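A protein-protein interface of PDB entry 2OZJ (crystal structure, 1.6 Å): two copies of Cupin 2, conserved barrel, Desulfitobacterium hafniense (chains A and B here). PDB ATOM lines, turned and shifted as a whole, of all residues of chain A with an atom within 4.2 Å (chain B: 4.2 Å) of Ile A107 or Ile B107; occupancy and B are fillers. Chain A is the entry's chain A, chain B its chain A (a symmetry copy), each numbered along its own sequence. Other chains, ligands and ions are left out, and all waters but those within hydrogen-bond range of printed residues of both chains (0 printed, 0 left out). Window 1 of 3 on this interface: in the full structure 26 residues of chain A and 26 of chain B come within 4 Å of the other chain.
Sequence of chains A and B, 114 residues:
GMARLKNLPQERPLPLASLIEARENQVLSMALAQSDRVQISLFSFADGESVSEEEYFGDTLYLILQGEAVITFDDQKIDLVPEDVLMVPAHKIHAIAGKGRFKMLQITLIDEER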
ATOM      1  N   VAL A  38      -4.563  23.942 -19.056  1.00  0.00           N
ATOM      2  CA  VAL A  38      -4.213  25.220 -19.669  1.00  0.00           C
ATOM      3  C   VAL A  38      -3.752  24.983 -21.087  1.00  0.00           C
ATOM      4  O   VAL A  38      -3.018  24.022 -21.387  1.00  0.00           O
ATOM      5  CB  VAL A  38      -3.180  26.059 -18.847  1.00  0.00           C
ATOM      6  CG1 VAL A  38      -1.797  25.417 -18.837  1.00  0.00           C
ATOM      7  CG2 VAL A  38      -3.088  27.493 -19.383  1.00  0.00           C
ATOM      8  N   GLN A  39      -4.226  25.855 -21.963  1.00  0.00           N
ATOM      9  CA  GLN A  39      -3.789  25.888 -23.329  1.00  0.00           C
ATOM     10  C   GLN A  39      -2.948  27.153 -23.491  1.00  0.00           C
ATOM     11  O   GLN A  39      -3.372  28.248 -23.149  1.00  0.00           O
ATOM     12  CB  GLN A  39      -5.000  25.904 -24.248  1.00  0.00           C
ATOM     13  CG  GLN A  39      -5.830  24.596 -24.231  1.00  0.00           C
ATOM     14  CD  GLN A  39      -6.930  24.534 -25.343  1.00  0.00           C
ATOM     15  N   ILE A  40      -1.736  26.985 -24.009  1.00  0.00           N
ATOM     16  CA  ILE A  40      -0.832  28.101 -24.252  1.00  0.00           C
ATOM     17  C   ILE A  40      -0.364  27.942 -25.682  1.00  0.00           C
ATOM     18  O   ILE A  40       0.238  26.898 -26.034  1.00  0.00           O
ATOM     19  CB  ILE A  40       0.392  28.117 -23.284  1.00  0.00           C
ATOM     20  CG1 ILE A  40      -0.055  27.950 -21.824  1.00  0.00           C
ATOM     21  CG2 ILE A  40       1.237  29.384 -23.555  1.00  0.00           C
ATOM     22  CD1 ILE A  40       1.134  27.972 -20.810  1.00  0.00           C
ATOM     23  N   ASP A  59     -11.342  31.459 -18.777  1.00  0.00           N
ATOM     24  CA  ASP A  59     -10.710  32.752 -19.019  1.00  0.00           C
ATOM     25  C   ASP A  59      -9.530  32.623 -19.967  1.00  0.00           C
ATOM     26  O   ASP A  59      -8.827  31.614 -19.958  1.00  0.00           O
ATOM     27  CB  ASP A  59     -10.232  33.363 -17.698  1.00  0.00           C
ATOM     28  CG  ASP A  59     -11.352  33.712 -16.749  1.00  0.00           C
ATOM     29  OD1 ASP A  59     -12.525  33.780 -17.139  1.00  0.00           O
ATOM     30  OD2 ASP A  59     -11.017  33.952 -15.569  1.00  0.00           O
ATOM     31  N   THR A  60      -9.320  33.670 -20.763  1.00  0.00           N
ATOM     32  CA  THR A  60      -8.249  33.757 -21.736  1.00  0.00           C
ATOM     33  C   THR A  60      -7.519  35.051 -21.578  1.00  0.00           C
ATOM     34  O   THR A  60      -8.139  36.073 -21.324  1.00  0.00           O
ATOM     35  CB  THR A  60      -8.817  33.729 -23.151  1.00  0.00           C
ATOM     36  OG1 THR A  60      -9.550  32.524 -23.290  1.00  0.00           O
ATOM     37  CG2 THR A  60      -7.708  33.759 -24.192  1.00  0.00           C
ATOM     38  N   LEU A  61      -6.200  35.020 -21.662  1.00  0.00           N
ATOM     39  CA  LEU A  61      -5.428  36.246 -21.859  1.00  0.00           C
ATOM     40  C   LEU A  61      -4.744  36.214 -23.211  1.00  0.00           C
ATOM     41  O   LEU A  61      -4.127  35.218 -23.604  1.00  0.00           O
ATOM     42  CB  LEU A  61      -4.407  36.493 -20.754  1.00  0.00           C
ATOM     43  CG  LEU A  61      -3.007  35.863 -20.697  1.00  0.00           C
ATOM     44  CD1 LEU A  61      -2.067  36.402 -21.803  1.00  0.00           C
ATOM     45  CD2 LEU A  61      -2.360  36.106 -19.340  1.00  0.00           C
ATOM     46  N   GLN A 106      -1.618  33.301 -26.654  1.00  0.00           N
ATOM     47  CA  GLN A 106      -2.914  33.083 -26.025  1.00  0.00           C
ATOM     48  C   GLN A 106      -2.720  32.105 -24.872  1.00  0.00           C
ATOM     49  O   GLN A 106      -2.036  31.088 -25.019  1.00  0.00           O
ATOM     50  CB  GLN A 106      -3.888  32.481 -27.033  1.00  0.00           C
ATOM     51  CG  GLN A 106      -5.222  32.040 -26.446  1.00  0.00           C
ATOM     52  CD  GLN A 106      -6.248  31.643 -27.517  1.00  0.00           C
ATOM     53  OE1 GLN A 106      -6.086  31.950 -28.692  1.00  0.00           O
ATOM     54  NE2 GLN A 106      -7.301  30.957 -27.092  1.00  0.00           N
ATOM     55  N   ILE A 107      -3.308  32.427 -23.729  1.00  0.00           N
ATOM     56  CA  ILE A 107      -3.365  31.506 -22.596  1.00  0.00           C
ATOM     57  C   ILE A 107      -4.807  31.336 -22.232  1.00  0.00           C
ATOM     58  O   ILE A 107      -5.462  32.306 -21.927  1.00  0.00           O
ATOM     59  CB  ILE A 107      -2.568  32.031 -21.377  1.00  0.00           C
ATOM     60  CG1 ILE A 107      -1.098  32.185 -21.736  1.00  0.00           C
ATOM     61  CG2 ILE A 107      -2.764  31.065 -20.137  1.00  0.00           C
ATOM     62  CD1 ILE A 107      -0.346  33.050 -20.716  1.00  0.00           C
ATOM     63  N   THR A 108      -5.314  30.113 -22.319  1.00  0.00           N
ATOM     64  CA  THR A 108      -6.692  29.838 -21.964  1.00  0.00           C
ATOM     65  C   THR A 108      -6.788  28.753 -20.895  1.00  0.00           C
ATOM     66  O   THR A 108      -6.177  27.698 -21.018  1.00  0.00           O
ATOM     67  CB  THR A 108      -7.542  29.460 -23.181  1.00  0.00           C
ATOM     68  OG1 THR A 108      -7.486  30.501 -24.145  1.00  0.00           O
ATOM     69  CG2 THR A 108      -8.985  29.283 -22.767  1.00  0.00           C
ATOM     70  N   VAL B  38      -1.977  25.940 -12.527  1.00  0.00           N
ATOM     71  CA  VAL B  38      -1.005  26.860 -13.110  1.00  0.00           C
ATOM     72  C   VAL B  38      -0.878  28.077 -12.225  1.00  0.00           C
ATOM     73  O   VAL B  38      -1.870  28.607 -11.691  1.00  0.00           O
ATOM     74  CB  VAL B  38      -1.304  27.244 -14.597  1.00  0.00           C
ATOM     75  CG1 VAL B  38      -2.553  28.107 -14.729  1.00  0.00           C
ATOM     76  CG2 VAL B  38      -0.104  27.958 -15.230  1.00  0.00           C
ATOM     77  N   GLN B  39       0.368  28.488 -12.048  1.00  0.00           N
ATOM     78  CA  GLN B  39       0.684  29.709 -11.364  1.00  0.00           C
ATOM     79  C   GLN B  39       1.192  30.687 -12.423  1.00  0.00           C
ATOM     80  O   GLN B  39       2.091  30.381 -13.194  1.00  0.00           O
ATOM     81  CB  GLN B  39       1.742  29.438 -10.306  1.00  0.00           C
ATOM     82  CG  GLN B  39       1.255  28.554  -9.130  1.00  0.00           C
ATOM     83  CD  GLN B  39       2.269  28.473  -7.941  1.00  0.00           C
ATOM     84  N   ILE B  40       0.591  31.871 -12.457  1.00  0.00           N
ATOM     85  CA  ILE B  40       0.987  32.917 -13.391  1.00  0.00           C
ATOM     86  C   ILE B  40       1.172  34.163 -12.552  1.00  0.00           C
ATOM     87  O   ILE B  40       0.213  34.615 -11.878  1.00  0.00           O
ATOM     88  CB  ILE B  40      -0.074  33.173 -14.507  1.00  0.00           C
ATOM     89  CG1 ILE B  40      -0.519  31.856 -15.158  1.00  0.00           C
ATOM     90  CG2 ILE B  40       0.475  34.226 -15.498  1.00  0.00           C
ATOM     91  CD1 ILE B  40      -1.574  32.057 -16.294  1.00  0.00           C
ATOM     92  N   ASP B  59       7.189  22.393 -14.967  1.00  0.00           N
ATOM     93  CA  ASP B  59       7.866  23.278 -15.910  1.00  0.00           C
ATOM     94  C   ASP B  59       7.480  24.729 -15.682  1.00  0.00           C
ATOM     95  O   ASP B  59       6.349  25.025 -15.303  1.00  0.00           O
ATOM     96  CB  ASP B  59       7.518  22.883 -17.348  1.00  0.00           C
ATOM     97  CG  ASP B  59       8.029  21.520 -17.746  1.00  0.00           C
ATOM     98  OD1 ASP B  59       8.892  20.939 -17.077  1.00  0.00           O
ATOM     99  OD2 ASP B  59       7.548  21.038 -18.794  1.00  0.00           O
ATOM    100  N   THR B  60       8.436  25.621 -15.940  1.00  0.00           N
ATOM    101  CA  THR B  60       8.280  27.055 -15.795  1.00  0.00           C
ATOM    102  C   THR B  60       8.744  27.748 -17.034  1.00  0.00           C
ATOM    103  O   THR B  60       9.735  27.342 -17.624  1.00  0.00           O
ATOM    104  CB  THR B  60       9.138  27.566 -14.643  1.00  0.00           C
ATOM    105  OG1 THR B  60       8.732  26.876 -13.472  1.00  0.00           O
ATOM    106  CG2 THR B  60       8.944  29.060 -14.431  1.00  0.00           C
ATOM    107  N   LEU B  61       8.011  28.753 -17.480  1.00  0.00           N
ATOM    108  CA  LEU B  61       8.542  29.696 -18.463  1.00  0.00           C
ATOM    109  C   LEU B  61       8.667  31.073 -17.842  1.00  0.00           C
ATOM    110  O   LEU B  61       7.752  31.573 -17.180  1.00  0.00           O
ATOM    111  CB  LEU B  61       7.709  29.763 -19.738  1.00  0.00           C
ATOM    112  CG  LEU B  61       6.440  30.610 -19.914  1.00  0.00           C
ATOM    113  CD1 LEU B  61       6.738  32.130 -19.927  1.00  0.00           C
ATOM    114  CD2 LEU B  61       5.716  30.239 -21.200  1.00  0.00           C
ATOM    115  N   GLN B 106       6.149  34.999 -14.951  1.00  0.00           N
ATOM    116  CA  GLN B 106       6.474  33.602 -14.701  1.00  0.00           C
ATOM    117  C   GLN B 106       5.201  32.783 -14.877  1.00  0.00           C
ATOM    118  O   GLN B 106       4.135  33.165 -14.384  1.00  0.00           O
ATOM    119  CB  GLN B 106       6.985  33.432 -13.274  1.00  0.00           C
ATOM    120  CG  GLN B 106       7.185  31.988 -12.835  1.00  0.00           C
ATOM    121  CD  GLN B 106       7.898  31.865 -11.481  1.00  0.00           C
ATOM    122  OE1 GLN B 106       8.494  32.817 -10.991  1.00  0.00           O
ATOM    123  NE2 GLN B 106       7.828  30.680 -10.887  1.00  0.00           N
ATOM    124  N   ILE B 107       5.314  31.673 -15.590  1.00  0.00           N
ATOM    125  CA  ILE B 107       4.231  30.697 -15.691  1.00  0.00           C
ATOM    126  C   ILE B 107       4.778  29.377 -15.244  1.00  0.00           C
ATOM    127  O   ILE B 107       5.730  28.902 -15.819  1.00  0.00           O
ATOM    128  CB  ILE B 107       3.681  30.583 -17.134  1.00  0.00           C
ATOM    129  CG1 ILE B 107       3.106  31.917 -17.585  1.00  0.00           C
ATOM    130  CG2 ILE B 107       2.602  29.427 -17.220  1.00  0.00           C
ATOM    131  CD1 ILE B 107       2.907  31.972 -19.105  1.00  0.00           C
ATOM    132  N   THR B 108       4.210  28.813 -14.186  1.00  0.00           N
ATOM    133  CA  THR B 108       4.648  27.524 -13.690  1.00  0.00           C
ATOM    134  C   THR B 108       3.494  26.528 -13.626  1.00  0.00           C
ATOM    135  O   THR B 108       2.432  26.833 -13.096  1.00  0.00           O
ATOM    136  CB  THR B 108       5.333  27.628 -12.323  1.00  0.00           C
ATOM    137  OG1 THR B 108       6.438  28.517 -12.409  1.00  0.00           O
ATOM    138  CG2 THR B 108       5.856  26.273 -11.904  1.00  0.00           C
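The backbone carbonyl oxygen (O) of Ile A107 lies within hydrogen-bond range of the backbone NH (N) of Leu A61, 2.8 Å away.
N of Leu B61 lies within hydrogen-bond range of O of Ile B107.
Among the printed residues, merely in contact across the chains: Ile A107 with Ile B107.
Of chain B, only Ile B107 (3.8 Å) comes within 4 Å of Ile A107.
Gln B39 touches none of the printed residues of chain A.
Thr B60 touches none of the printed residues of chain A.
Ile B107 touches one residue of chain A.
The nearest residue of chain B that does not touch Ile A107 is Ile B40 (4.1 Å).
Hydrophobic or aromatic side chains of chain A within 4 Å of the printed part of chain B: Ile A107.
Of the 9 printed residues of chain B, 1 touches a printed residue of chain A.
Printed residues of chain B that touch a printed residue of chain A: Ile B107.
Hydrophobic or aromatic side chains of chain B that line the printed part of chain A: Ile B107.
Among the printed residues, no Asp or Glu carboxylate lies within 4 Å of a Lys or Arg side-chain nitrogen of the other chain.
Ile A107 touches its own counterpart, Ile B107.
9 positions are printed for both chains.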
